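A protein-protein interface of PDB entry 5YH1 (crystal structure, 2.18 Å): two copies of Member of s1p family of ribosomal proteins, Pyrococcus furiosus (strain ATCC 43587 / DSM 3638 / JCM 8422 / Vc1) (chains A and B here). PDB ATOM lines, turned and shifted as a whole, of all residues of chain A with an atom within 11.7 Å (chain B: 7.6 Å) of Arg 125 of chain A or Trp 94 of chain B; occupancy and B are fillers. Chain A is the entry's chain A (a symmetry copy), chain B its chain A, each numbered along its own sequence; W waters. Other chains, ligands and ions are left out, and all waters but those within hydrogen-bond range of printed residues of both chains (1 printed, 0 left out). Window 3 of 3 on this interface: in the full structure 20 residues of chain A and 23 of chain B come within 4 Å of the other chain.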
ATOM      1  N   PRO A  57     -19.703   1.321  13.364  1.00  0.00           N
ATOM      2  CA  PRO A  57     -19.497   0.203  14.280  1.00  0.00           C
ATOM      3  C   PRO A  57     -20.599  -0.838  14.193  1.00  0.00           C
ATOM      4  O   PRO A  57     -21.697  -0.551  13.713  1.00  0.00           O
ATOM      5  CB  PRO A  57     -19.487   0.852  15.673  1.00  0.00           C
ATOM      6  CG  PRO A  57     -20.041   2.214  15.508  1.00  0.00           C
ATOM      7  CD  PRO A  57     -19.937   2.598  14.063  1.00  0.00           C
ATOM      8  N   HIS A  95     -12.309  -1.318  18.057  1.00  0.00           N
ATOM      9  CA  HIS A  95     -13.258  -0.263  18.333  1.00  0.00           C
ATOM     10  C   HIS A  95     -14.569  -0.403  17.552  1.00  0.00           C
ATOM     11  O   HIS A  95     -15.633  -0.099  18.082  1.00  0.00           O
ATOM     12  CB  HIS A  95     -12.626   1.090  18.037  1.00  0.00           C
ATOM     13  CG  HIS A  95     -13.513   2.234  18.379  1.00  0.00           C
ATOM     14  ND1 HIS A  95     -13.984   2.443  19.655  1.00  0.00           N
ATOM     15  CD2 HIS A  95     -14.054   3.207  17.610  1.00  0.00           C
ATOM     16  CE1 HIS A  95     -14.766   3.507  19.664  1.00  0.00           C
ATOM     17  NE2 HIS A  95     -14.821   3.990  18.435  1.00  0.00           N
ATOM     18  N   ILE A 116     -27.151   0.718  24.293  1.00  0.00           N
ATOM     19  CA  ILE A 116     -27.520   2.096  23.963  1.00  0.00           C
ATOM     20  C   ILE A 116     -26.621   3.109  24.702  1.00  0.00           C
ATOM     21  O   ILE A 116     -26.139   4.071  24.110  1.00  0.00           O
ATOM     22  CB  ILE A 116     -29.024   2.349  24.231  1.00  0.00           C
ATOM     23  CG1 ILE A 116     -29.860   1.548  23.228  1.00  0.00           C
ATOM     24  CG2 ILE A 116     -29.373   3.841  24.107  1.00  0.00           C
ATOM     25  CD1 ILE A 116     -31.338   1.457  23.566  1.00  0.00           C
ATOM     26  N   ILE A 117     -26.363   2.887  25.981  1.00  0.00           N
ATOM     27  CA  ILE A 117     -25.510   3.816  26.741  1.00  0.00           C
ATOM     28  C   ILE A 117     -24.103   3.833  26.153  1.00  0.00           C
ATOM     29  O   ILE A 117     -23.532   4.896  25.926  1.00  0.00           O
ATOM     30  CB  ILE A 117     -25.491   3.458  28.242  1.00  0.00           C
ATOM     31  CG1 ILE A 117     -26.869   3.739  28.849  1.00  0.00           C
ATOM     32  CG2 ILE A 117     -24.393   4.228  28.990  1.00  0.00           C
ATOM     33  CD1 ILE A 117     -27.179   2.951  30.102  1.00  0.00           C
ATOM     34  N   PHE A 118     -23.557   2.655  25.879  1.00  0.00           N
ATOM     35  CA  PHE A 118     -22.223   2.536  25.295  1.00  0.00           C
ATOM     36  C   PHE A 118     -22.153   3.175  23.910  1.00  0.00           C
ATOM     37  O   PHE A 118     -21.212   3.901  23.618  1.00  0.00           O
ATOM     38  CB  PHE A 118     -21.788   1.062  25.227  1.00  0.00           C
ATOM     39  CG  PHE A 118     -21.139   0.546  26.490  1.00  0.00           C
ATOM     40  CD1 PHE A 118     -21.530   0.995  27.755  1.00  0.00           C
ATOM     41  CD2 PHE A 118     -20.138  -0.417  26.415  1.00  0.00           C
ATOM     42  CE1 PHE A 118     -20.922   0.501  28.907  1.00  0.00           C
ATOM     43  CE2 PHE A 118     -19.528  -0.914  27.567  1.00  0.00           C
ATOM     44  CZ  PHE A 118     -19.922  -0.449  28.815  1.00  0.00           C
ATOM     45  N   MET A 119     -23.135   2.910  23.050  1.00  0.00           N
ATOM     46  CA  MET A 119     -23.103   3.473  21.685  1.00  0.00           C
ATOM     47  C   MET A 119     -23.268   4.982  21.714  1.00  0.00           C
ATOM     48  O   MET A 119     -22.669   5.686  20.904  1.00  0.00           O
ATOM     49  CB  MET A 119     -24.128   2.802  20.756  1.00  0.00           C
ATOM     50  CG  MET A 119     -25.543   3.319  20.990  1.00  0.00           C
ATOM     51  SD  MET A 119     -26.943   2.484  19.870  1.00  0.00           S
ATOM     52  CE  MET A 119     -26.790   0.601  20.421  1.00  0.00           C
ATOM     53  N   MET A 120     -24.072   5.496  22.642  1.00  0.00           N
ATOM     54  CA  MET A 120     -24.270   6.943  22.745  1.00  0.00           C
ATOM     55  C   MET A 120     -23.014   7.622  23.260  1.00  0.00           C
ATOM     56  O   MET A 120     -22.699   8.738  22.852  1.00  0.00           O
ATOM     57  CB  MET A 120     -25.488   7.262  23.611  1.00  0.00           C
ATOM     58  CG  MET A 120     -26.801   7.026  22.869  1.00  0.00           C
ATOM     59  SD  MET A 120     -26.914   8.118  21.224  1.00  0.00           S
ATOM     60  CE  MET A 120     -26.661   9.904  22.035  1.00  0.00           C
ATOM     61  N   GLU A 121     -22.260   6.960  24.131  1.00  0.00           N
ATOM     62  CA  GLU A 121     -20.984   7.534  24.567  1.00  0.00           C
ATOM     63  C   GLU A 121     -19.982   7.649  23.415  1.00  0.00           C
ATOM     64  O   GLU A 121     -19.339   8.680  23.255  1.00  0.00           O
ATOM     65  CB  GLU A 121     -20.353   6.736  25.708  1.00  0.00           C
ATOM     66  CG  GLU A 121     -19.002   7.314  26.097  1.00  0.00           C
ATOM     67  CD  GLU A 121     -18.492   6.830  27.431  1.00  0.00           C
ATOM     68  OE1 GLU A 121     -19.304   6.578  28.339  1.00  0.00           O
ATOM     69  OE2 GLU A 121     -17.265   6.720  27.573  1.00  0.00           O
ATOM     70  N   ASP A 122     -19.822   6.580  22.639  1.00  0.00           N
ATOM     71  CA  ASP A 122     -18.931   6.618  21.475  1.00  0.00           C
ATOM     72  C   ASP A 122     -19.382   7.672  20.465  1.00  0.00           C
ATOM     73  O   ASP A 122     -18.555   8.363  19.873  1.00  0.00           O
ATOM     74  CB  ASP A 122     -18.847   5.247  20.801  1.00  0.00           C
ATOM     75  CG  ASP A 122     -17.994   4.263  21.575  1.00  0.00           C
ATOM     76  OD1 ASP A 122     -17.258   4.656  22.502  1.00  0.00           O
ATOM     77  OD2 ASP A 122     -18.052   3.073  21.249  1.00  0.00           O
ATOM     78  N   HIS A 123     -20.688   7.780  20.269  1.00  0.00           N
ATOM     79  CA  HIS A 123     -21.247   8.798  19.403  1.00  0.00           C
ATOM     80  C   HIS A 123     -20.850  10.207  19.863  1.00  0.00           C
ATOM     81  O   HIS A 123     -20.252  10.962  19.109  1.00  0.00           O
ATOM     82  CB  HIS A 123     -22.765   8.670  19.364  1.00  0.00           C
ATOM     83  CG  HIS A 123     -23.429   9.616  18.415  1.00  0.00           C
ATOM     84  ND1 HIS A 123     -23.174   9.611  17.060  1.00  0.00           N
ATOM     85  CD2 HIS A 123     -24.348  10.588  18.623  1.00  0.00           C
ATOM     86  CE1 HIS A 123     -23.911  10.536  16.473  1.00  0.00           C
ATOM     87  NE2 HIS A 123     -24.632  11.144  17.398  1.00  0.00           N
ATOM     88  N   MET A 124     -21.148  10.533  21.113  1.00  0.00           N
ATOM     89  CA  MET A 124     -20.920  11.883  21.632  1.00  0.00           C
ATOM     90  C   MET A 124     -19.459  12.163  21.824  1.00  0.00           C
ATOM     91  O   MET A 124     -18.991  13.253  21.534  1.00  0.00           O
ATOM     92  CB  MET A 124     -21.610  12.064  22.979  1.00  0.00           C
ATOM     93  CG  MET A 124     -23.131  12.014  22.857  1.00  0.00           C
ATOM     94  SD  MET A 124     -23.980  12.082  24.645  1.00  0.00           S
ATOM     95  CE  MET A 124     -23.512  10.351  25.443  1.00  0.00           C
ATOM     96  N   ARG A 125     -18.711  11.186  22.307  1.00  0.00           N
ATOM     97  CA  ARG A 125     -17.317  11.424  22.680  1.00  0.00           C
ATOM     98  C   ARG A 125     -16.352  11.382  21.491  1.00  0.00           C
ATOM     99  O   ARG A 125     -15.437  12.195  21.412  1.00  0.00           O
ATOM    100  CB  ARG A 125     -16.905  10.406  23.731  1.00  0.00           C
ATOM    101  CG  ARG A 125     -15.610  10.712  24.440  1.00  0.00           C
ATOM    102  CD  ARG A 125     -15.401   9.708  25.548  1.00  0.00           C
ATOM    103  NE  ARG A 125     -14.218  10.025  26.330  1.00  0.00           N
ATOM    104  CZ  ARG A 125     -13.924   9.480  27.504  1.00  0.00           C
ATOM    105  NH1 ARG A 125     -14.726   8.584  28.059  1.00  0.00           N
ATOM    106  NH2 ARG A 125     -12.822   9.844  28.133  1.00  0.00           N
ATOM    107  N   PHE A 126     -16.548  10.433  20.579  1.00  0.00           N
ATOM    108  CA  PHE A 126     -15.632  10.253  19.451  1.00  0.00           C
ATOM    109  C   PHE A 126     -16.258  10.549  18.090  1.00  0.00           C
ATOM    110  O   PHE A 126     -15.579  10.452  17.086  1.00  0.00           O
ATOM    111  CB  PHE A 126     -15.072   8.831  19.453  1.00  0.00           C
ATOM    112  CG  PHE A 126     -14.463   8.431  20.760  1.00  0.00           C
ATOM    113  CD1 PHE A 126     -13.312   9.056  21.221  1.00  0.00           C
ATOM    114  CD2 PHE A 126     -15.042   7.437  21.539  1.00  0.00           C
ATOM    115  CE1 PHE A 126     -12.751   8.694  22.435  1.00  0.00           C
ATOM    116  CE2 PHE A 126     -14.483   7.075  22.751  1.00  0.00           C
ATOM    117  CZ  PHE A 126     -13.341   7.704  23.203  1.00  0.00           C
ATOM    118  N   GLY A 127     -17.542  10.895  18.049  1.00  0.00           N
ATOM    119  CA  GLY A 127     -18.222  11.174  16.780  1.00  0.00           C
ATOM    120  C   GLY A 127     -18.559   9.947  15.943  1.00  0.00           C
ATOM    121  O   GLY A 127     -18.925  10.085  14.779  1.00  0.00           O
ATOM    122  N   ASP A 128     -18.445   8.748  16.515  1.00  0.00           N
ATOM    123  CA  ASP A 128     -18.843   7.521  15.812  1.00  0.00           C
ATOM    124  C   ASP A 128     -20.311   7.572  15.412  1.00  0.00           C
ATOM    125  O   ASP A 128     -21.151   8.085  16.155  1.00  0.00           O
ATOM    126  CB  ASP A 128     -18.664   6.286  16.703  1.00  0.00           C
ATOM    127  CG  ASP A 128     -17.223   5.974  17.007  1.00  0.00           C
ATOM    128  OD1 ASP A 128     -16.343   6.318  16.205  1.00  0.00           O
ATOM    129  OD2 ASP A 128     -16.962   5.369  18.062  1.00  0.00           O
ATOM    130  N   GLU A 129     -20.625   7.015  14.252  1.00  0.00           N
ATOM    131  CA  GLU A 129     -22.012   6.752  13.899  1.00  0.00           C
ATOM    132  C   GLU A 129     -22.591   5.715  14.858  1.00  0.00           C
ATOM    133  O   GLU A 129     -21.859   4.945  15.487  1.00  0.00           O
ATOM    134  CB  GLU A 129     -22.107   6.213  12.472  1.00  0.00           C
ATOM    135  CG  GLU A 129     -21.650   7.174  11.389  1.00  0.00           C
ATOM    136  CD  GLU A 129     -22.705   8.198  11.042  1.00  0.00           C
ATOM    137  OE1 GLU A 129     -23.047   9.025  11.906  1.00  0.00           O
ATOM    138  OE2 GLU A 129     -23.197   8.179   9.897  1.00  0.00           O
ATOM    139  N   LEU A 130     -23.911   5.694  14.965  1.00  0.00           N
ATOM    140  CA  LEU A 130     -24.591   4.671  15.738  1.00  0.00           C
ATOM    141  C   LEU A 130     -24.460   3.331  15.003  1.00  0.00           C
ATOM    142  O   LEU A 130     -24.423   3.288  13.771  1.00  0.00           O
ATOM    143  CB  LEU A 130     -26.051   5.036  15.956  1.00  0.00           C
ATOM    144  CG  LEU A 130     -26.302   6.325  16.746  1.00  0.00           C
ATOM    145  CD1 LEU A 130     -27.797   6.508  16.940  1.00  0.00           C
ATOM    146  CD2 LEU A 130     -25.587   6.342  18.086  1.00  0.00           C
ATOM    147  N   GLU B  76     -25.673  18.144  36.456  1.00  0.00           N
ATOM    148  CA  GLU B  76     -24.787  17.815  35.334  1.00  0.00           C
ATOM    149  C   GLU B  76     -24.977  18.781  34.160  1.00  0.00           C
ATOM    150  O   GLU B  76     -24.003  19.207  33.514  1.00  0.00           O
ATOM    151  CB  GLU B  76     -25.006  16.347  34.888  1.00  0.00           C
ATOM    152  CG  GLU B  76     -24.286  15.954  33.605  1.00  0.00           C
ATOM    153  CD  GLU B  76     -24.341  14.458  33.281  1.00  0.00           C
ATOM    154  OE1 GLU B  76     -24.015  14.102  32.136  1.00  0.00           O
ATOM    155  OE2 GLU B  76     -24.680  13.625  34.142  1.00  0.00           O
ATOM    156  N   ILE B  80     -21.478  20.686  33.069  1.00  0.00           N
ATOM    157  CA  ILE B  80     -20.732  20.269  31.870  1.00  0.00           C
ATOM    158  C   ILE B  80     -20.346  21.447  30.960  1.00  0.00           C
ATOM    159  O   ILE B  80     -19.189  21.539  30.548  1.00  0.00           O
ATOM    160  CB  ILE B  80     -21.489  19.180  31.061  1.00  0.00           C
ATOM    161  CG1 ILE B  80     -21.549  17.853  31.831  1.00  0.00           C
ATOM    162  CG2 ILE B  80     -20.859  18.962  29.695  1.00  0.00           C
ATOM    163  CD1 ILE B  80     -20.211  17.280  32.225  1.00  0.00           C
ATOM    164  N   ILE B  83     -17.420  23.347  32.461  1.00  0.00           N
ATOM    165  CA  ILE B  83     -16.203  22.561  32.300  1.00  0.00           C
ATOM    166  C   ILE B  83     -15.661  22.703  30.881  1.00  0.00           C
ATOM    167  O   ILE B  83     -14.454  22.858  30.688  1.00  0.00           O
ATOM    168  CB  ILE B  83     -16.434  21.072  32.634  1.00  0.00           C
ATOM    169  CG1 ILE B  83     -16.634  20.903  34.143  1.00  0.00           C
ATOM    170  CG2 ILE B  83     -15.266  20.214  32.145  1.00  0.00           C
ATOM    171  CD1 ILE B  83     -17.081  19.515  34.554  1.00  0.00           C
ATOM    172  N   GLU B  84     -16.556  22.657  29.898  1.00  0.00           N
ATOM    173  CA  GLU B  84     -16.154  22.737  28.495  1.00  0.00           C
ATOM    174  C   GLU B  84     -15.642  24.119  28.086  1.00  0.00           C
ATOM    175  O   GLU B  84     -14.766  24.211  27.226  1.00  0.00           O
ATOM    176  CB  GLU B  84     -17.280  22.255  27.567  1.00  0.00           C
ATOM    177  CG  GLU B  84     -17.485  20.746  27.670  1.00  0.00           C
ATOM    178  CD  GLU B  84     -18.458  20.180  26.656  1.00  0.00           C
ATOM    179  OE1 GLU B  84     -19.483  20.843  26.370  1.00  0.00           O
ATOM    180  OE2 GLU B  84     -18.196  19.060  26.158  1.00  0.00           O
ATOM    181  N   ASP B  89      -8.820  20.783  26.669  1.00  0.00           N
ATOM    182  CA  ASP B  89      -9.043  19.407  26.221  1.00  0.00           C
ATOM    183  C   ASP B  89     -10.542  19.124  25.999  1.00  0.00           C
ATOM    184  O   ASP B  89     -11.360  19.410  26.872  1.00  0.00           O
ATOM    185  CB  ASP B  89      -8.472  18.446  27.280  1.00  0.00           C
ATOM    186  CG  ASP B  89      -8.215  17.046  26.748  1.00  0.00           C
ATOM    187  OD1 ASP B  89      -8.501  16.766  25.566  1.00  0.00           O
ATOM    188  OD2 ASP B  89      -7.716  16.212  27.531  1.00  0.00           O
ATOM    189  N   PRO B  90     -10.912  18.567  24.828  1.00  0.00           N
ATOM    190  CA  PRO B  90     -12.305  18.123  24.642  1.00  0.00           C
ATOM    191  C   PRO B  90     -12.684  16.852  25.422  1.00  0.00           C
ATOM    192  O   PRO B  90     -13.867  16.518  25.510  1.00  0.00           O
ATOM    193  CB  PRO B  90     -12.394  17.865  23.132  1.00  0.00           C
ATOM    194  CG  PRO B  90     -10.987  17.620  22.703  1.00  0.00           C
ATOM    195  CD  PRO B  90     -10.153  18.517  23.565  1.00  0.00           C
ATOM    196  N   GLU B  91     -11.696  16.149  25.969  1.00  0.00           N
ATOM    197  CA  GLU B  91     -11.948  15.011  26.855  1.00  0.00           C
ATOM    198  C   GLU B  91     -12.264  15.443  28.301  1.00  0.00           C
ATOM    199  O   GLU B  91     -12.672  14.618  29.117  1.00  0.00           O
ATOM    200  CB  GLU B  91     -10.745  14.054  26.840  1.00  0.00           C
ATOM    201  CG  GLU B  91     -10.568  13.290  25.530  1.00  0.00           C
ATOM    202  CD  GLU B  91     -11.304  11.958  25.515  1.00  0.00           C
ATOM    203  OE1 GLU B  91     -10.857  11.025  26.216  1.00  0.00           O
ATOM    204  OE2 GLU B  91     -12.324  11.831  24.805  1.00  0.00           O
ATOM    205  N   ALA B  92     -12.090  16.728  28.610  1.00  0.00           N
ATOM    206  CA  ALA B  92     -12.291  17.241  29.972  1.00  0.00           C
ATOM    207  C   ALA B  92     -13.682  16.965  30.554  1.00  0.00           C
ATOM    208  O   ALA B  92     -13.801  16.563  31.711  1.00  0.00           O
ATOM    209  CB  ALA B  92     -12.002  18.728  30.014  1.00  0.00           C
ATOM    210  N   ARG B  93     -14.721  17.198  29.757  1.00  0.00           N
ATOM    211  CA  ARG B  93     -16.091  16.836  30.129  1.00  0.00           C
ATOM    212  C   ARG B  93     -16.168  15.427  30.700  1.00  0.00           C
ATOM    213  O   ARG B  93     -16.757  15.201  31.759  1.00  0.00           O
ATOM    214  CB  ARG B  93     -17.022  16.904  28.914  1.00  0.00           C
ATOM    215  CG  ARG B  93     -18.173  15.908  29.002  1.00  0.00           C
ATOM    216  CD  ARG B  93     -19.105  15.980  27.823  1.00  0.00           C
ATOM    217  NE  ARG B  93     -20.363  15.307  28.132  1.00  0.00           N
ATOM    218  CZ  ARG B  93     -21.471  15.440  27.413  1.00  0.00           C
ATOM    219  NH1 ARG B  93     -21.477  16.212  26.326  1.00  0.00           N
ATOM    220  NH2 ARG B  93     -22.573  14.794  27.772  1.00  0.00           N
ATOM    221  N   TRP B  94     -15.585  14.481  29.974  1.00  0.00           N
ATOM    222  CA  TRP B  94     -15.728  13.066  30.289  1.00  0.00           C
ATOM    223  C   TRP B  94     -14.868  12.687  31.467  1.00  0.00           C
ATOM    224  O   TRP B  94     -15.214  11.801  32.236  1.00  0.00           O
ATOM    225  CB  TRP B  94     -15.377  12.213  29.061  1.00  0.00           C
ATOM    226  CG  TRP B  94     -16.302  12.518  27.938  1.00  0.00           C
ATOM    227  CD1 TRP B  94     -16.104  13.410  26.926  1.00  0.00           C
ATOM    228  CD2 TRP B  94     -17.614  11.990  27.762  1.00  0.00           C
ATOM    229  NE1 TRP B  94     -17.209  13.450  26.112  1.00  0.00           N
ATOM    230  CE2 TRP B  94     -18.153  12.588  26.606  1.00  0.00           C
ATOM    231  CE3 TRP B  94     -18.387  11.058  28.470  1.00  0.00           C
ATOM    232  CZ2 TRP B  94     -19.427  12.284  26.134  1.00  0.00           C
ATOM    233  CZ3 TRP B  94     -19.657  10.752  28.001  1.00  0.00           C
ATOM    234  CH2 TRP B  94     -20.164  11.367  26.844  1.00  0.00           C
ATOM    235  N   HIS B  95     -13.746  13.368  31.614  1.00  0.00           N
ATOM    236  CA  HIS B  95     -12.787  13.006  32.634  1.00  0.00           C
ATOM    237  C   HIS B  95     -13.027  13.711  33.973  1.00  0.00           C
ATOM    238  O   HIS B  95     -12.831  13.111  35.025  1.00  0.00           O
ATOM    239  CB  HIS B  95     -11.376  13.300  32.144  1.00  0.00           C
ATOM    240  CG  HIS B  95     -10.324  12.873  33.107  1.00  0.00           C
ATOM    241  ND1 HIS B  95     -10.189  11.566  33.515  1.00  0.00           N
ATOM    242  CD2 HIS B  95      -9.387  13.580  33.778  1.00  0.00           C
ATOM    243  CE1 HIS B  95      -9.200  11.481  34.386  1.00  0.00           C
ATOM    244  NE2 HIS B  95      -8.695  12.690  34.560  1.00  0.00           N
ATOM    245  N   LEU B  96     -13.437  14.977  33.927  1.00  0.00           N
ATOM    246  CA  LEU B  96     -13.518  15.814  35.123  1.00  0.00           C
ATOM    247  C   LEU B  96     -14.922  15.884  35.749  1.00  0.00           C
ATOM    248  O   LEU B  96     -15.152  16.637  36.709  1.00  0.00           O
ATOM    249  CB  LEU B  96     -13.001  17.216  34.805  1.00  0.00           C
ATOM    250  CG  LEU B  96     -11.530  17.294  34.391  1.00  0.00           C
ATOM    251  CD1 LEU B  96     -11.181  18.710  33.965  1.00  0.00           C
ATOM    252  CD2 LEU B  96     -10.619  16.829  35.515  1.00  0.00           C
ATOM    253  N   PHE B  97     -15.852  15.096  35.216  1.00  0.00           N
ATOM    254  CA  PHE B  97     -17.153  14.934  35.839  1.00  0.00           C
ATOM    255  C   PHE B  97     -17.667  13.505  35.711  1.00  0.00           C
ATOM    256  O   PHE B  97     -17.704  12.946  34.614  1.00  0.00           O
ATOM    257  CB  PHE B  97     -18.173  15.897  35.240  1.00  0.00           C
ATOM    258  CG  PHE B  97     -19.541  15.766  35.844  1.00  0.00           C
ATOM    259  CD1 PHE B  97     -19.860  16.436  37.008  1.00  0.00           C
ATOM    260  CD2 PHE B  97     -20.500  14.948  35.258  1.00  0.00           C
ATOM    261  CE1 PHE B  97     -21.108  16.312  37.583  1.00  0.00           C
ATOM    262  CE2 PHE B  97     -21.756  14.819  35.827  1.00  0.00           C
ATOM    263  CZ  PHE B  97     -22.058  15.504  36.989  1.00  0.00           C
ATOM    264  N   LYS B  98     -18.094  12.941  36.837  1.00  0.00           N
ATOM    265  CA  LYS B  98     -18.680  11.612  36.881  1.00  0.00           C
ATOM    266  C   LYS B  98     -19.975  11.627  37.679  1.00  0.00           C
ATOM    267  O   LYS B  98     -20.010  12.139  38.793  1.00  0.00           O
ATOM    268  CB  LYS B  98     -17.706  10.635  37.540  1.00  0.00           C
ATOM    269  CG  LYS B  98     -16.418  10.425  36.765  1.00  0.00           C
ATOM    270  CD  LYS B  98     -16.686   9.633  35.491  1.00  0.00           C
ATOM    271  CE  LYS B  98     -15.573   9.817  34.476  1.00  0.00           C
ATOM    272  NZ  LYS B  98     -14.289   9.279  34.964  1.00  0.00           N
ATOM    273  N   ASP B 271     -25.525   4.777  34.496  1.00  0.00           N
ATOM    274  CA  ASP B 271     -26.089   6.091  34.827  1.00  0.00           C
ATOM    275  C   ASP B 271     -27.123   6.603  33.824  1.00  0.00           C
ATOM    276  O   ASP B 271     -27.685   7.676  34.013  1.00  0.00           O
ATOM    277  CB  ASP B 271     -24.976   7.125  35.024  1.00  0.00           C
ATOM    278  CG  ASP B 271     -24.136   7.346  33.787  1.00  0.00           C
ATOM    279  OD1 ASP B 271     -24.600   7.082  32.651  1.00  0.00           O
ATOM    280  OD2 ASP B 271     -22.991   7.817  33.959  1.00  0.00           O
ATOM    281  N   ARG B 273     -26.819   7.775  30.828  1.00  0.00           N
ATOM    282  CA  ARG B 273     -26.417   8.865  29.926  1.00  0.00           C
ATOM    283  C   ARG B 273     -26.695   8.472  28.476  1.00  0.00           C
ATOM    284  O   ARG B 273     -26.337   7.375  28.051  1.00  0.00           O
ATOM    285  CB  ARG B 273     -24.934   9.214  30.101  1.00  0.00           C
ATOM    286  CG  ARG B 273     -24.435  10.290  29.156  1.00  0.00           C
ATOM    287  CD  ARG B 273     -23.043  10.804  29.516  1.00  0.00           C
ATOM    288  NE  ARG B 273     -22.973  11.291  30.897  1.00  0.00           N
ATOM    289  CZ  ARG B 273     -22.524  10.589  31.944  1.00  0.00           C
ATOM    290  NH1 ARG B 273     -22.068   9.338  31.805  1.00  0.00           N
ATOM    291  NH2 ARG B 273     -22.525  11.138  33.161  1.00  0.00           N
ATOM    292  N   GLY B 274     -27.332   9.380  27.742  1.00  0.00           N
ATOM    293  CA  GLY B 274     -27.752   9.149  26.368  1.00  0.00           C
ATOM    294  C   GLY B 274     -29.212   8.770  26.289  1.00  0.00           C
ATOM    295  O   GLY B 274     -29.810   8.829  25.212  1.00  0.00           O
HETATM  296  O   HOH W   1     -23.767   7.339  27.111  1.00  0.00           O
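Of the 17 printed residues of chain A, 5 touch a printed residue of chain B. Hydrophobic or aromatic side chains of chain A that line the printed part of chain B: Ile 117, Met 124 and Phe 126. Among the printed residues, 7 pairs touch across the chains.
The side-chain carboxylate (OE1) of Glu 76 of chain B is in salt-bridge range of the guanidinium group (NE) of Arg 273 of chain B (3.2 Å). The side-chain carboxylate (OD1) of Asp 89 of chain B sits close to the backbone NH (N) of Glu 91 of chain B, 3.3 Å away. The side-chain carboxylate of Asp 271 of chain B lies within salt-bridge range of the guanidinium group of Arg 273 of chain B (2.8 Å). NH1 of Arg 125 of chain A lies within salt-bridge range of OE2 of Glu 121 of chain A, at 3.2 Å.
Of chain B, only Glu 91 and Trp 94 come within 4 Å of Arg 125 of chain A. Printed residues of chain A within 4 Å of Trp 94 of chain B: Glu 121 (3.98 Å), Met 124 (3.8 Å) and Arg 125 (3.5 Å). Of chain A, only Arg 125 and Phe 126 come within 4 Å of Glu 91 of chain B. No residue of chain A comes within 4 Å of Ala 92 of chain B. Arg 93 of chain B touches none of the printed residues of chain A. No residue of chain A comes within 4 Å of His 95 of chain B. Of the printed residues of chain B, Glu 121 of chain A touches Trp 94 (3.98 Å). Of the printed residues of chain B, Phe 126 of chain A touches Glu 91 (3.95 Å). Met 119 of chain A touches none of the printed residues of chain B. The nearest printed residue of chain B that does not touch Ile 117 of chain A is Asp 271 of chain B (4.6 Å).
Among the printed residues, pairs that only touch across the chains: Ile 117 of chain A with Arg 273 of chain B (3.8 Å), Glu 121 of chain A with Trp 94 of chain B (3.98 Å), Met 124 of chain A with Trp 94 of chain B (3.8 Å), Met 124 of chain A with Arg 273 of chain B (3.8 Å), Arg 125 of chain A with Trp 94 of chain B (3.5 Å) and Phe 126 of chain A with Glu 91 of chain B (3.95 Å).
The side-chain carboxylate (OE1) of Glu 91 of chain B lies within salt-bridge range of the guanidinium group (NH2) of Arg 125 of chain A, 3.0 Å away.
Water W1 lies within hydrogen-bond range of the backbone carbonyl oxygen (O) of Ile 117 of chain A, the backbone carbonyl oxygen (O) of Arg 273 of chain B and the backbone NH (N) of Glu 121 of chain A.
1 position is printed for both chains. Of the 7 pairs that touch across the chains among the printed residues, none has its exchanged pair printed and touching as well.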
